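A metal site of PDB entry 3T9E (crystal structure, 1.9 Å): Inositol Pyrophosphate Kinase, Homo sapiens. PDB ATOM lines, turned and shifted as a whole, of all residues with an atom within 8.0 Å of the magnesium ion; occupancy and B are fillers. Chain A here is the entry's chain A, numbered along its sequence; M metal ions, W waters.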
ATOM      1  N   GLN A   7     -24.419 -21.012  10.852  1.00  0.00           N
ATOM      2  CA  GLN A   7     -22.994 -21.056  11.178  1.00  0.00           C
ATOM      3  C   GLN A   7     -22.188 -20.154  10.261  1.00  0.00           C
ATOM      4  O   GLN A   7     -22.535 -19.973   9.099  1.00  0.00           O
ATOM      5  CB  GLN A   7     -22.484 -22.482  10.963  1.00  0.00           C
ATOM      6  CG  GLN A   7     -22.993 -23.489  11.968  1.00  0.00           C
ATOM      7  CD  GLN A   7     -22.350 -23.300  13.315  1.00  0.00           C
ATOM      8  OE1 GLN A   7     -22.918 -22.679  14.201  1.00  0.00           O
ATOM      9  NE2 GLN A   7     -21.130 -23.812  13.473  1.00  0.00           N
ATOM     10  N   ILE A   8     -21.093 -19.599  10.784  1.00  0.00           N
ATOM     11  CA  ILE A   8     -20.130 -18.887   9.946  1.00  0.00           C
ATOM     12  C   ILE A   8     -19.238 -19.961   9.356  1.00  0.00           C
ATOM     13  O   ILE A   8     -18.664 -20.768  10.085  1.00  0.00           O
ATOM     14  CB  ILE A   8     -19.307 -17.870  10.765  1.00  0.00           C
ATOM     15  CG1 ILE A   8     -20.204 -16.769  11.342  1.00  0.00           C
ATOM     16  CG2 ILE A   8     -18.196 -17.252   9.898  1.00  0.00           C
ATOM     17  CD1 ILE A   8     -19.623 -16.092  12.578  1.00  0.00           C
ATOM     18  N   LEU A  28      -7.218 -26.745  12.627  1.00  0.00           N
ATOM     19  CA  LEU A  28      -8.615 -26.760  12.210  1.00  0.00           C
ATOM     20  C   LEU A  28      -9.525 -27.391  13.252  1.00  0.00           C
ATOM     21  O   LEU A  28     -10.650 -26.924  13.470  1.00  0.00           O
ATOM     22  CB  LEU A  28      -8.782 -27.422  10.843  1.00  0.00           C
ATOM     23  CG  LEU A  28      -8.044 -26.720   9.684  1.00  0.00           C
ATOM     24  CD1 LEU A  28      -8.404 -27.450   8.435  1.00  0.00           C
ATOM     25  CD2 LEU A  28      -8.419 -25.226   9.584  1.00  0.00           C
ATOM     26  N   GLU A  29      -9.037 -28.414  13.946  1.00  0.00           N
ATOM     27  CA  GLU A  29      -9.825 -29.044  14.996  1.00  0.00           C
ATOM     28  C   GLU A  29     -10.100 -28.055  16.133  1.00  0.00           C
ATOM     29  O   GLU A  29     -11.167 -28.095  16.734  1.00  0.00           O
ATOM     30  CB  GLU A  29      -9.187 -30.336  15.503  1.00  0.00           C
ATOM     31  CG  GLU A  29      -7.923 -30.164  16.335  1.00  0.00           C
ATOM     32  CD  GLU A  29      -7.280 -31.487  16.702  1.00  0.00           C
ATOM     33  OE1 GLU A  29      -6.140 -31.466  17.228  1.00  0.00           O
ATOM     34  OE2 GLU A  29      -7.898 -32.548  16.478  1.00  0.00           O
ATOM     35  N   ARG A  30      -9.150 -27.159  16.399  1.00  0.00           N
ATOM     36  CA  ARG A  30      -9.322 -26.138  17.428  1.00  0.00           C
ATOM     37  C   ARG A  30     -10.242 -25.001  16.953  1.00  0.00           C
ATOM     38  O   ARG A  30     -11.070 -24.490  17.723  1.00  0.00           O
ATOM     39  CB  ARG A  30      -7.958 -25.624  17.889  1.00  0.00           C
ATOM     40  CG  ARG A  30      -7.149 -26.646  18.664  1.00  0.00           C
ATOM     41  CD  ARG A  30      -5.685 -26.291  18.596  1.00  0.00           C
ATOM     42  NE  ARG A  30      -4.866 -27.008  19.570  1.00  0.00           N
ATOM     43  CZ  ARG A  30      -4.377 -28.233  19.386  1.00  0.00           C
ATOM     44  NH1 ARG A  30      -4.631 -28.920  18.266  1.00  0.00           N
ATOM     45  NH2 ARG A  30      -3.628 -28.785  20.331  1.00  0.00           N
ATOM     46  N   ILE A  31     -10.111 -24.592  15.701  1.00  0.00           N
ATOM     47  CA  ILE A  31     -11.024 -23.575  15.158  1.00  0.00           C
ATOM     48  C   ILE A  31     -12.475 -24.068  15.219  1.00  0.00           C
ATOM     49  O   ILE A  31     -13.398 -23.305  15.525  1.00  0.00           O
ATOM     50  CB  ILE A  31     -10.657 -23.164  13.710  1.00  0.00           C
ATOM     51  CG1 ILE A  31      -9.300 -22.458  13.684  1.00  0.00           C
ATOM     52  CG2 ILE A  31     -11.755 -22.285  13.086  1.00  0.00           C
ATOM     53  CD1 ILE A  31      -8.806 -22.082  12.282  1.00  0.00           C
ATOM     54  N   SER A  32     -12.665 -25.354  14.932  1.00  0.00           N
ATOM     55  CA  SER A  32     -13.979 -25.971  14.991  1.00  0.00           C
ATOM     56  C   SER A  32     -14.636 -25.935  16.382  1.00  0.00           C
ATOM     57  O   SER A  32     -15.848 -26.097  16.499  1.00  0.00           O
ATOM     58  CB  SER A  32     -13.890 -27.414  14.506  1.00  0.00           C
ATOM     59  OG  SER A  32     -13.777 -27.446  13.103  1.00  0.00           O
ATOM     60  N   LEU A  33     -13.831 -25.700  17.420  1.00  0.00           N
ATOM     61  CA  LEU A  33     -14.355 -25.583  18.789  1.00  0.00           C
ATOM     62  C   LEU A  33     -15.153 -24.299  18.988  1.00  0.00           C
ATOM     63  O   LEU A  33     -15.947 -24.207  19.933  1.00  0.00           O
ATOM     64  CB  LEU A  33     -13.241 -25.652  19.839  1.00  0.00           C
ATOM     65  CG  LEU A  33     -12.403 -26.922  20.000  1.00  0.00           C
ATOM     66  CD1 LEU A  33     -11.182 -26.627  20.862  1.00  0.00           C
ATOM     67  CD2 LEU A  33     -13.208 -28.091  20.567  1.00  0.00           C
ATOM     68  N   PHE A  34     -14.966 -23.308  18.107  1.00  0.00           N
ATOM     69  CA  PHE A  34     -15.797 -22.118  18.166  1.00  0.00           C
ATOM     70  C   PHE A  34     -17.251 -22.504  17.874  1.00  0.00           C
ATOM     71  O   PHE A  34     -17.550 -23.124  16.833  1.00  0.00           O
ATOM     72  CB  PHE A  34     -15.308 -21.007  17.215  1.00  0.00           C
ATOM     73  CG  PHE A  34     -14.133 -20.226  17.740  1.00  0.00           C
ATOM     74  CD1 PHE A  34     -12.863 -20.807  17.804  1.00  0.00           C
ATOM     75  CD2 PHE A  34     -14.290 -18.899  18.151  1.00  0.00           C
ATOM     76  CE1 PHE A  34     -11.774 -20.079  18.286  1.00  0.00           C
ATOM     77  CE2 PHE A  34     -13.206 -18.157  18.623  1.00  0.00           C
ATOM     78  CZ  PHE A  34     -11.936 -18.743  18.700  1.00  0.00           C
ATOM     79  N   LYS A  35     -18.132 -22.164  18.807  1.00  0.00           N
ATOM     80  CA  LYS A  35     -19.544 -22.550  18.749  1.00  0.00           C
ATOM     81  C   LYS A  35     -20.221 -22.231  17.421  1.00  0.00           C
ATOM     82  O   LYS A  35     -21.004 -23.041  16.914  1.00  0.00           O
ATOM     83  CB  LYS A  35     -20.326 -21.884  19.910  1.00  0.00           C
ATOM     84  CG  LYS A  35     -21.810 -22.274  19.972  1.00  0.00           C
ATOM     85  CD  LYS A  35     -22.493 -21.807  21.269  1.00  0.00           C
ATOM     86  CE  LYS A  35     -21.965 -22.571  22.499  1.00  0.00           C
ATOM     87  NZ  LYS A  35     -22.944 -22.576  23.649  1.00  0.00           N
ATOM     88  N   TYR A  36     -19.914 -21.059  16.857  1.00  0.00           N
ATOM     89  CA  TYR A  36     -20.591 -20.544  15.670  1.00  0.00           C
ATOM     90  C   TYR A  36     -19.803 -20.658  14.378  1.00  0.00           C
ATOM     91  O   TYR A  36     -20.174 -20.063  13.364  1.00  0.00           O
ATOM     92  CB  TYR A  36     -21.000 -19.090  15.880  1.00  0.00           C
ATOM     93  CG  TYR A  36     -21.979 -18.912  17.009  1.00  0.00           C
ATOM     94  CD1 TYR A  36     -23.337 -19.220  16.837  1.00  0.00           C
ATOM     95  CD2 TYR A  36     -21.557 -18.458  18.267  1.00  0.00           C
ATOM     96  CE1 TYR A  36     -24.256 -19.065  17.897  1.00  0.00           C
ATOM     97  CE2 TYR A  36     -22.459 -18.303  19.326  1.00  0.00           C
ATOM     98  CZ  TYR A  36     -23.812 -18.609  19.125  1.00  0.00           C
ATOM     99  OH  TYR A  36     -24.702 -18.443  20.173  1.00  0.00           O
ATOM    100  N   ILE A  37     -18.713 -21.405  14.410  1.00  0.00           N
ATOM    101  CA  ILE A  37     -17.884 -21.560  13.230  1.00  0.00           C
ATOM    102  C   ILE A  37     -17.916 -23.000  12.762  1.00  0.00           C
ATOM    103  O   ILE A  37     -17.770 -23.910  13.567  1.00  0.00           O
ATOM    104  CB  ILE A  37     -16.412 -21.142  13.503  1.00  0.00           C
ATOM    105  CG1 ILE A  37     -16.330 -19.625  13.720  1.00  0.00           C
ATOM    106  CG2 ILE A  37     -15.492 -21.581  12.336  1.00  0.00           C
ATOM    107  CD1 ILE A  37     -14.930 -19.109  14.038  1.00  0.00           C
ATOM    108  N   THR A  38     -18.108 -23.204  11.462  1.00  0.00           N
ATOM    109  CA  THR A  38     -17.950 -24.505  10.819  1.00  0.00           C
ATOM    110  C   THR A  38     -16.803 -24.400   9.819  1.00  0.00           C
ATOM    111  O   THR A  38     -16.743 -23.455   9.042  1.00  0.00           O
ATOM    112  CB  THR A  38     -19.234 -24.921  10.070  1.00  0.00           C
ATOM    113  OG1 THR A  38     -20.316 -24.984  11.002  1.00  0.00           O
ATOM    114  CG2 THR A  38     -19.046 -26.289   9.424  1.00  0.00           C
ATOM    115  N   VAL A  39     -15.914 -25.386   9.845  1.00  0.00           N
ATOM    116  CA  VAL A  39     -14.781 -25.441   8.951  1.00  0.00           C
ATOM    117  C   VAL A  39     -15.100 -26.381   7.796  1.00  0.00           C
ATOM    118  O   VAL A  39     -15.604 -27.498   8.012  1.00  0.00           O
ATOM    119  CB  VAL A  39     -13.516 -25.891   9.714  1.00  0.00           C
ATOM    120  CG1 VAL A  39     -12.357 -26.155   8.786  1.00  0.00           C
ATOM    121  CG2 VAL A  39     -13.146 -24.838  10.752  1.00  0.00           C
HETATM  122 MG    MG M   1     -17.630 -25.026  15.428  1.00  0.00          MG
HETATM  123  O   HOH W   1     -19.789 -25.306  15.111  1.00  0.00           O
HETATM  124  O   HOH W   2     -17.930 -26.910  14.166  1.00  0.00           O
HETATM  125  O   HOH W   3     -18.667 -26.234  18.007  1.00  0.00           O
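NE2 of Gln 7 sits close to O of Ile 37.
The side-chain hydroxyl (OG) of Ser 32 sits at hydrogen-bond distance from the backbone carbonyl oxygen (O) of Leu 28 (3.2 Å).
Within 4 Å of the magnesium ion: Ser 32, Phe 34 and Ile 37.
The nearest printed residue that does not touch the magnesium ion is Lys 35 (4.2 Å).
The magnesium ion is bound by the backbone carbonyl oxygen (O) of Ile 37 (2.2 Å).
The magnesium ion is bound by water W1, at 2.2 Å.
Water W2 is bound to the magnesium ion (2.3 Å).
O of Ser 32 binds the magnesium ion.
O of Phe 34 binds the magnesium ion, at 2.4 Å.
Water W1 bridges NE2 of Gln 7 (2.6 Å) and O of Lys 35 (3.1 Å).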
